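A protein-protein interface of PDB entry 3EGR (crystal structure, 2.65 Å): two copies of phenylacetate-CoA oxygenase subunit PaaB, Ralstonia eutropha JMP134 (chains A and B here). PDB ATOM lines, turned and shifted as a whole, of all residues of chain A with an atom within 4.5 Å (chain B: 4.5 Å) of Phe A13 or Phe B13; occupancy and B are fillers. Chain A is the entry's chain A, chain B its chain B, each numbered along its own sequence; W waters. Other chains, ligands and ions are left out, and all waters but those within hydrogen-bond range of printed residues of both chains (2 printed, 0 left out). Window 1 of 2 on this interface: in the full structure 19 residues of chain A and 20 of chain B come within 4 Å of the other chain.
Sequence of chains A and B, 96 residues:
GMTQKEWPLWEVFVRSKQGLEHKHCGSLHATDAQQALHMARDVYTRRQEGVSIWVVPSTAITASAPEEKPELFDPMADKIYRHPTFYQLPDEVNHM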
ATOM      1  N   GLU A  11      19.111 -29.676  -2.228  1.00  0.00           N
ATOM      2  CA  GLU A  11      20.400 -30.014  -1.656  1.00  0.00           C
ATOM      3  C   GLU A  11      20.384 -29.640  -0.180  1.00  0.00           C
ATOM      4  O   GLU A  11      19.807 -28.611   0.213  1.00  0.00           O
ATOM      5  CB  GLU A  11      21.534 -29.299  -2.385  1.00  0.00           C
ATOM      6  CG  GLU A  11      21.637 -29.624  -3.874  1.00  0.00           C
ATOM      7  CD  GLU A  11      21.759 -31.099  -4.156  1.00  0.00           C
ATOM      8  OE1 GLU A  11      22.327 -31.847  -3.329  1.00  0.00           O
ATOM      9  OE2 GLU A  11      21.297 -31.516  -5.228  1.00  0.00           O
ATOM     10  N   VAL A  12      21.011 -30.491   0.627  1.00  0.00           N
ATOM     11  CA  VAL A  12      21.000 -30.353   2.070  1.00  0.00           C
ATOM     12  C   VAL A  12      22.422 -30.089   2.565  1.00  0.00           C
ATOM     13  O   VAL A  12      23.352 -30.828   2.235  1.00  0.00           O
ATOM     14  CB  VAL A  12      20.473 -31.651   2.717  1.00  0.00           C
ATOM     15  CG1 VAL A  12      20.512 -31.576   4.243  1.00  0.00           C
ATOM     16  CG2 VAL A  12      19.073 -31.941   2.228  1.00  0.00           C
ATOM     17  N   PHE A  13      22.576 -29.050   3.378  1.00  0.00           N
ATOM     18  CA  PHE A  13      23.854 -28.718   4.000  1.00  0.00           C
ATOM     19  C   PHE A  13      23.631 -28.667   5.495  1.00  0.00           C
ATOM     20  O   PHE A  13      22.654 -28.063   5.940  1.00  0.00           O
ATOM     21  CB  PHE A  13      24.360 -27.352   3.523  1.00  0.00           C
ATOM     22  CG  PHE A  13      24.421 -27.211   2.023  1.00  0.00           C
ATOM     23  CD1 PHE A  13      23.282 -26.921   1.292  1.00  0.00           C
ATOM     24  CD2 PHE A  13      25.613 -27.360   1.344  1.00  0.00           C
ATOM     25  CE1 PHE A  13      23.333 -26.793  -0.079  1.00  0.00           C
ATOM     26  CE2 PHE A  13      25.663 -27.236  -0.031  1.00  0.00           C
ATOM     27  CZ  PHE A  13      24.521 -26.956  -0.738  1.00  0.00           C
ATOM     28  N   VAL A  14      24.540 -29.278   6.261  1.00  0.00           N
ATOM     29  CA  VAL A  14      24.433 -29.330   7.720  1.00  0.00           C
ATOM     30  C   VAL A  14      25.691 -28.792   8.401  1.00  0.00           C
ATOM     31  O   VAL A  14      26.807 -29.026   7.939  1.00  0.00           O
ATOM     32  CB  VAL A  14      24.221 -30.768   8.204  1.00  0.00           C
ATOM     33  CG1 VAL A  14      24.353 -30.830   9.698  1.00  0.00           C
ATOM     34  CG2 VAL A  14      22.873 -31.277   7.767  1.00  0.00           C
ATOM     35  N   ARG A  15      25.508 -28.065   9.498  1.00  0.00           N
ATOM     36  CA  ARG A  15      26.619 -27.695  10.354  1.00  0.00           C
ATOM     37  C   ARG A  15      26.371 -28.296  11.709  1.00  0.00           C
ATOM     38  O   ARG A  15      25.412 -27.938  12.377  1.00  0.00           O
ATOM     39  CB  ARG A  15      26.735 -26.188  10.493  1.00  0.00           C
ATOM     40  CG  ARG A  15      27.927 -25.753  11.317  1.00  0.00           C
ATOM     41  CD  ARG A  15      27.925 -24.262  11.489  1.00  0.00           C
ATOM     42  NE  ARG A  15      26.791 -23.834  12.302  1.00  0.00           N
ATOM     43  CZ  ARG A  15      26.219 -22.631  12.245  1.00  0.00           C
ATOM     44  NH1 ARG A  15      26.662 -21.682  11.421  1.00  0.00           N
ATOM     45  NH2 ARG A  15      25.181 -22.374  13.035  1.00  0.00           N
ATOM     46  N   HIS A  22      28.838 -25.174   7.262  1.00  0.00           N
ATOM     47  CA  HIS A  22      27.856 -26.077   6.686  1.00  0.00           C
ATOM     48  C   HIS A  22      28.532 -26.931   5.605  1.00  0.00           C
ATOM     49  O   HIS A  22      29.230 -26.398   4.750  1.00  0.00           O
ATOM     50  CB  HIS A  22      26.677 -25.284   6.097  1.00  0.00           C
ATOM     51  CG  HIS A  22      25.740 -24.718   7.128  1.00  0.00           C
ATOM     52  ND1 HIS A  22      25.991 -23.541   7.800  1.00  0.00           N
ATOM     53  CD2 HIS A  22      24.538 -25.161   7.583  1.00  0.00           C
ATOM     54  CE1 HIS A  22      24.991 -23.291   8.633  1.00  0.00           C
ATOM     55  NE2 HIS A  22      24.095 -24.257   8.518  1.00  0.00           N
ATOM     56  N   LYS A  23      28.350 -28.250   5.677  1.00  0.00           N
ATOM     57  CA  LYS A  23      28.893 -29.193   4.696  1.00  0.00           C
ATOM     58  C   LYS A  23      27.716 -29.851   3.970  1.00  0.00           C
ATOM     59  O   LYS A  23      26.714 -30.225   4.592  1.00  0.00           O
ATOM     60  CB  LYS A  23      29.765 -30.287   5.360  1.00  0.00           C
ATOM     61  CG  LYS A  23      30.953 -29.787   6.224  1.00  0.00           C
ATOM     62  CD  LYS A  23      31.838 -30.922   6.820  1.00  0.00           C
ATOM     63  N   HIS A  24      27.839 -29.987   2.653  1.00  0.00           N
ATOM     64  CA  HIS A  24      26.843 -30.686   1.852  1.00  0.00           C
ATOM     65  C   HIS A  24      26.841 -32.145   2.232  1.00  0.00           C
ATOM     66  O   HIS A  24      27.887 -32.790   2.211  1.00  0.00           O
ATOM     67  CB  HIS A  24      27.181 -30.564   0.373  1.00  0.00           C
ATOM     68  CG  HIS A  24      26.186 -31.211  -0.533  1.00  0.00           C
ATOM     69  ND1 HIS A  24      26.549 -32.118  -1.505  1.00  0.00           N
ATOM     70  CD2 HIS A  24      24.843 -31.063  -0.637  1.00  0.00           C
ATOM     71  CE1 HIS A  24      25.468 -32.511  -2.158  1.00  0.00           C
ATOM     72  NE2 HIS A  24      24.421 -31.882  -1.656  1.00  0.00           N
ATOM     73  N   SER A  52      22.691 -27.031  12.688  1.00  0.00           N
ATOM     74  CA  SER A  52      22.007 -26.153  11.723  1.00  0.00           C
ATOM     75  C   SER A  52      21.851 -26.848  10.385  1.00  0.00           C
ATOM     76  O   SER A  52      22.832 -27.375   9.857  1.00  0.00           O
ATOM     77  CB  SER A  52      22.790 -24.864  11.502  1.00  0.00           C
ATOM     78  OG  SER A  52      22.171 -24.031  10.530  1.00  0.00           O
ATOM     79  N   ILE A  53      20.630 -26.824   9.840  1.00  0.00           N
ATOM     80  CA  ILE A  53      20.343 -27.386   8.518  1.00  0.00           C
ATOM     81  C   ILE A  53      19.964 -26.297   7.504  1.00  0.00           C
ATOM     82  O   ILE A  53      19.122 -25.448   7.773  1.00  0.00           O
ATOM     83  CB  ILE A  53      19.176 -28.428   8.571  1.00  0.00           C
ATOM     84  CG1 ILE A  53      19.340 -29.371   9.770  1.00  0.00           C
ATOM     85  CG2 ILE A  53      19.088 -29.229   7.256  1.00  0.00           C
ATOM     86  CD1 ILE A  53      18.166 -30.350   9.957  1.00  0.00           C
ATOM     87  N   TRP A  54      20.586 -26.339   6.333  1.00  0.00           N
ATOM     88  CA  TRP A  54      20.192 -25.511   5.190  1.00  0.00           C
ATOM     89  C   TRP A  54      19.699 -26.400   4.059  1.00  0.00           C
ATOM     90  O   TRP A  54      20.378 -27.370   3.685  1.00  0.00           O
ATOM     91  CB  TRP A  54      21.371 -24.704   4.652  1.00  0.00           C
ATOM     92  CG  TRP A  54      21.846 -23.586   5.509  1.00  0.00           C
ATOM     93  CD1 TRP A  54      21.293 -23.151   6.675  1.00  0.00           C
ATOM     94  CD2 TRP A  54      22.951 -22.714   5.236  1.00  0.00           C
ATOM     95  NE1 TRP A  54      21.996 -22.071   7.158  1.00  0.00           N
ATOM     96  CE2 TRP A  54      23.018 -21.782   6.293  1.00  0.00           C
ATOM     97  CE3 TRP A  54      23.893 -22.632   4.202  1.00  0.00           C
ATOM     98  CZ2 TRP A  54      23.994 -20.786   6.353  1.00  0.00           C
ATOM     99  CZ3 TRP A  54      24.863 -21.633   4.256  1.00  0.00           C
ATOM    100  CH2 TRP A  54      24.909 -20.731   5.332  1.00  0.00           C
ATOM    101  N   VAL A  56      18.238 -26.121  -0.020  1.00  0.00           N
ATOM    102  CA  VAL A  56      18.292 -25.284  -1.213  1.00  0.00           C
ATOM    103  C   VAL A  56      17.756 -26.089  -2.384  1.00  0.00           C
ATOM    104  O   VAL A  56      18.210 -27.220  -2.622  1.00  0.00           O
ATOM    105  CB  VAL A  56      19.738 -24.894  -1.551  1.00  0.00           C
ATOM    106  CG1 VAL A  56      19.751 -23.861  -2.625  1.00  0.00           C
ATOM    107  CG2 VAL A  56      20.442 -24.400  -0.304  1.00  0.00           C
ATOM    108  N   GLU B  11      25.937 -17.214  -1.561  1.00  0.00           N
ATOM    109  CA  GLU B  11      26.641 -18.079  -0.630  1.00  0.00           C
ATOM    110  C   GLU B  11      27.479 -19.015  -1.475  1.00  0.00           C
ATOM    111  O   GLU B  11      27.026 -19.493  -2.545  1.00  0.00           O
ATOM    112  CB  GLU B  11      25.655 -18.876   0.215  1.00  0.00           C
ATOM    113  CG  GLU B  11      24.698 -18.006   1.015  1.00  0.00           C
ATOM    114  CD  GLU B  11      25.362 -17.278   2.167  1.00  0.00           C
ATOM    115  OE1 GLU B  11      26.438 -17.726   2.650  1.00  0.00           O
ATOM    116  OE2 GLU B  11      24.795 -16.261   2.619  1.00  0.00           O
ATOM    117  N   VAL B  12      28.686 -19.290  -0.988  1.00  0.00           N
ATOM    118  CA  VAL B  12      29.664 -20.031  -1.760  1.00  0.00           C
ATOM    119  C   VAL B  12      30.108 -21.291  -1.038  1.00  0.00           C
ATOM    120  O   VAL B  12      30.535 -21.229   0.117  1.00  0.00           O
ATOM    121  CB  VAL B  12      30.893 -19.143  -2.032  1.00  0.00           C
ATOM    122  CG1 VAL B  12      31.925 -19.888  -2.883  1.00  0.00           C
ATOM    123  CG2 VAL B  12      30.448 -17.843  -2.691  1.00  0.00           C
ATOM    124  N   PHE B  13      30.029 -22.417  -1.749  1.00  0.00           N
ATOM    125  CA  PHE B  13      30.484 -23.726  -1.270  1.00  0.00           C
ATOM    126  C   PHE B  13      31.586 -24.228  -2.208  1.00  0.00           C
ATOM    127  O   PHE B  13      31.457 -24.131  -3.437  1.00  0.00           O
ATOM    128  CB  PHE B  13      29.324 -24.723  -1.234  1.00  0.00           C
ATOM    129  CG  PHE B  13      28.100 -24.193  -0.541  1.00  0.00           C
ATOM    130  CD1 PHE B  13      27.227 -23.339  -1.203  1.00  0.00           C
ATOM    131  CD2 PHE B  13      27.836 -24.522   0.779  1.00  0.00           C
ATOM    132  CE1 PHE B  13      26.110 -22.820  -0.560  1.00  0.00           C
ATOM    133  CE2 PHE B  13      26.732 -24.021   1.428  1.00  0.00           C
ATOM    134  CZ  PHE B  13      25.863 -23.163   0.764  1.00  0.00           C
ATOM    135  N   VAL B  14      32.664 -24.746  -1.622  1.00  0.00           N
ATOM    136  CA  VAL B  14      33.824 -25.226  -2.374  1.00  0.00           C
ATOM    137  C   VAL B  14      34.138 -26.666  -1.990  1.00  0.00           C
ATOM    138  O   VAL B  14      34.076 -27.014  -0.813  1.00  0.00           O
ATOM    139  CB  VAL B  14      35.077 -24.376  -2.062  1.00  0.00           C
ATOM    140  CG1 VAL B  14      36.265 -24.893  -2.809  1.00  0.00           C
ATOM    141  CG2 VAL B  14      34.832 -22.919  -2.418  1.00  0.00           C
ATOM    142  N   ARG B  15      34.444 -27.505  -2.977  1.00  0.00           N
ATOM    143  CA  ARG B  15      34.940 -28.850  -2.702  1.00  0.00           C
ATOM    144  C   ARG B  15      36.310 -28.927  -3.313  1.00  0.00           C
ATOM    145  O   ARG B  15      36.453 -28.817  -4.522  1.00  0.00           O
ATOM    146  CB  ARG B  15      34.046 -29.926  -3.299  1.00  0.00           C
ATOM    147  CG  ARG B  15      34.532 -31.340  -3.011  1.00  0.00           C
ATOM    148  CD  ARG B  15      33.824 -32.361  -3.866  1.00  0.00           C
ATOM    149  NE  ARG B  15      34.088 -32.132  -5.289  1.00  0.00           N
ATOM    150  CZ  ARG B  15      33.251 -32.440  -6.285  1.00  0.00           C
ATOM    151  NH1 ARG B  15      32.064 -32.999  -6.048  1.00  0.00           N
ATOM    152  NH2 ARG B  15      33.598 -32.186  -7.540  1.00  0.00           N
ATOM    153  N   HIS B  22      31.145 -30.448  -0.800  1.00  0.00           N
ATOM    154  CA  HIS B  22      31.224 -28.990  -0.814  1.00  0.00           C
ATOM    155  C   HIS B  22      31.041 -28.378   0.586  1.00  0.00           C
ATOM    156  O   HIS B  22      30.046 -28.629   1.240  1.00  0.00           O
ATOM    157  CB  HIS B  22      30.209 -28.416  -1.787  1.00  0.00           C
ATOM    158  CG  HIS B  22      30.517 -28.722  -3.211  1.00  0.00           C
ATOM    159  ND1 HIS B  22      30.348 -29.976  -3.753  1.00  0.00           N
ATOM    160  CD2 HIS B  22      30.980 -27.937  -4.210  1.00  0.00           C
ATOM    161  CE1 HIS B  22      30.694 -29.950  -5.029  1.00  0.00           C
ATOM    162  NE2 HIS B  22      31.084 -28.724  -5.333  1.00  0.00           N
ATOM    163  N   LYS B  23      32.024 -27.602   1.039  1.00  0.00           N
ATOM    164  CA  LYS B  23      31.961 -26.907   2.326  1.00  0.00           C
ATOM    165  C   LYS B  23      31.640 -25.443   2.051  1.00  0.00           C
ATOM    166  O   LYS B  23      32.177 -24.845   1.115  1.00  0.00           O
ATOM    167  CB  LYS B  23      33.298 -26.989   3.072  1.00  0.00           C
ATOM    168  CG  LYS B  23      33.788 -28.402   3.452  1.00  0.00           C
ATOM    169  CD  LYS B  23      35.111 -28.399   4.278  1.00  0.00           C
ATOM    170  N   HIS B  24      30.762 -24.866   2.863  1.00  0.00           N
ATOM    171  CA  HIS B  24      30.472 -23.435   2.803  1.00  0.00           C
ATOM    172  C   HIS B  24      31.718 -22.728   3.222  1.00  0.00           C
ATOM    173  O   HIS B  24      32.313 -23.087   4.234  1.00  0.00           O
ATOM    174  CB  HIS B  24      29.370 -23.072   3.787  1.00  0.00           C
ATOM    175  CG  HIS B  24      28.953 -21.633   3.735  1.00  0.00           C
ATOM    176  ND1 HIS B  24      29.021 -20.800   4.832  1.00  0.00           N
ATOM    177  CD2 HIS B  24      28.444 -20.887   2.722  1.00  0.00           C
ATOM    178  CE1 HIS B  24      28.575 -19.604   4.492  1.00  0.00           C
ATOM    179  NE2 HIS B  24      28.218 -19.630   3.221  1.00  0.00           N
ATOM    180  N   SER B  52      35.851 -27.587  -7.259  1.00  0.00           N
ATOM    181  CA  SER B  52      34.469 -27.340  -7.664  1.00  0.00           C
ATOM    182  C   SER B  52      33.853 -26.257  -6.778  1.00  0.00           C
ATOM    183  O   SER B  52      33.900 -26.344  -5.546  1.00  0.00           O
ATOM    184  CB  SER B  52      33.654 -28.627  -7.556  1.00  0.00           C
ATOM    185  OG  SER B  52      32.295 -28.398  -7.854  1.00  0.00           O
ATOM    186  N   ILE B  53      33.284 -25.239  -7.411  1.00  0.00           N
ATOM    187  CA  ILE B  53      32.638 -24.142  -6.699  1.00  0.00           C
ATOM    188  C   ILE B  53      31.145 -24.136  -7.004  1.00  0.00           C
ATOM    189  O   ILE B  53      30.733 -24.269  -8.170  1.00  0.00           O
ATOM    190  CB  ILE B  53      33.244 -22.776  -7.100  1.00  0.00           C
ATOM    191  CG1 ILE B  53      34.781 -22.831  -6.966  1.00  0.00           C
ATOM    192  CG2 ILE B  53      32.632 -21.650  -6.244  1.00  0.00           C
ATOM    193  CD1 ILE B  53      35.503 -21.558  -7.374  1.00  0.00           C
ATOM    194  N   TRP B  54      30.338 -24.017  -5.955  1.00  0.00           N
ATOM    195  CA  TRP B  54      28.915 -23.773  -6.118  1.00  0.00           C
ATOM    196  C   TRP B  54      28.571 -22.373  -5.587  1.00  0.00           C
ATOM    197  O   TRP B  54      29.018 -22.004  -4.497  1.00  0.00           O
ATOM    198  CB  TRP B  54      28.088 -24.787  -5.318  1.00  0.00           C
ATOM    199  CG  TRP B  54      28.067 -26.189  -5.810  1.00  0.00           C
ATOM    200  CD1 TRP B  54      28.588 -26.666  -6.965  1.00  0.00           C
ATOM    201  CD2 TRP B  54      27.438 -27.295  -5.163  1.00  0.00           C
ATOM    202  NE1 TRP B  54      28.334 -28.012  -7.079  1.00  0.00           N
ATOM    203  CE2 TRP B  54      27.626 -28.421  -5.983  1.00  0.00           C
ATOM    204  CE3 TRP B  54      26.726 -27.440  -3.968  1.00  0.00           C
ATOM    205  CZ2 TRP B  54      27.135 -29.674  -5.653  1.00  0.00           C
ATOM    206  CZ3 TRP B  54      26.235 -28.677  -3.641  1.00  0.00           C
ATOM    207  CH2 TRP B  54      26.437 -29.784  -4.487  1.00  0.00           C
ATOM    208  N   VAL B  56      25.063 -19.898  -4.724  1.00  0.00           N
ATOM    209  CA  VAL B  56      23.627 -19.871  -4.457  1.00  0.00           C
ATOM    210  C   VAL B  56      23.240 -18.506  -3.936  1.00  0.00           C
ATOM    211  O   VAL B  56      23.868 -18.018  -3.011  1.00  0.00           O
ATOM    212  CB  VAL B  56      23.251 -20.854  -3.333  1.00  0.00           C
ATOM    213  CG1 VAL B  56      21.781 -21.069  -3.333  1.00  0.00           C
ATOM    214  CG2 VAL B  56      23.971 -22.169  -3.517  1.00  0.00           C
HETATM  215  O   HOH W   1      29.136 -32.008  -2.177  1.00  0.00           O
HETATM  216  O   HOH W   2      28.506 -22.395   7.218  1.00  0.00           O
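N of His B24 is in hydrogen-bond range of O of His A22 (2.9 Å).
The backbone carbonyl oxygen of His B22 lies within hydrogen-bond range of the backbone NH of His A24, at 3.0 Å.
O of Val A56 is in hydrogen-bond range of N of Glu A11 (2.6 Å).
The backbone carbonyl oxygen (O) of Val A14 is in hydrogen-bond range of the backbone NH (N) of Lys A23 (2.8 Å).
OE1 of Glu B11 is in hydrogen-bond range of NE2 of His B24 (2.7 Å).
N of Glu B11 is in hydrogen-bond range of O of Val B56 (2.7 Å).
N of Trp B54 lies within hydrogen-bond range of O of Phe B13 (2.8 Å).
The side-chain hydroxyl of Ser B52 lies within hydrogen-bond range of a ring nitrogen (NE2) of His B22, 2.8 Å away.
Among the printed residues, pairs that only touch across the chains: Phe A13 with Phe B13 (3.5 Å), Phe A13 with Trp B54 (3.8 Å), His A22 with Lys B23 (3.7 Å), Lys A23 with His B22 (3.7 Å), His A24 with Trp B54 (3.7 Å), Trp A54 with Phe B13 (3.9 Å), Trp A54 with His B24 (3.9 Å) and Val A56 with Val B56 (3.5 Å).
Phe A13 touches just these residues of chain B: Phe B13 and Trp B54.
Of the printed residues of chain A, Phe B13 touches Phe A13 and Trp A54.
Printed residues of chain A within 4 Å of Lys B23: His A22.
Printed residues of chain A within 4 Å of His B22: Lys A23 and His A24.
Of the printed residues of chain A, His B24 touches His A22 (2.9 Å) and Trp A54 (3.9 Å).
Of the printed residues of chain B, Val A56 touches Val B56 (3.5 Å).
Ile B53 touches none of the printed residues of chain A.
The nearest printed residue of chain B that does not touch Phe A13 is His B22 (4.6 Å).
The nearest printed residue of chain B that does not touch His A22 is His B22 (4.2 Å).
Of the 12 printed residues of chain A, 6 touch a printed residue of chain B.
Hydrophobic or aromatic side chains of chain A within 4 Å of the printed part of chain B: Phe A13, His A24, Trp A54 and Val A56.
Of the 12 printed residues of chain B, 6 touch a printed residue of chain A.
Hydrophobic or aromatic side chains of chain B within 4 Å of the printed part of chain A: Phe B13, His B24, Trp B54 and Val B56.
Among the printed residues, 10 pairs touch across the chains.
Among the printed residues, no Asp or Glu carboxylate lies within 4 Å of a Lys or Arg side-chain nitrogen of the other chain.
Phe A13 touches its own counterpart, Phe B13.
Phe A13 touches Trp B54, and with the chains exchanged Trp A54 touches Phe B13.
His A22 touches Lys B23, and with the chains exchanged Lys A23 touches His B22.
His A22 touches His B24, and with the chains exchanged His A24 touches His B22.
Water W1 bridges a ring nitrogen (ND1) of His A24 (2.7 Å) and a ring nitrogen (ND1) of His B22 (2.8 Å).
Water W2 bridges the backbone NH of His A22 (2.8 Å) and a ring nitrogen (ND1) of His B24 (2.9 Å).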
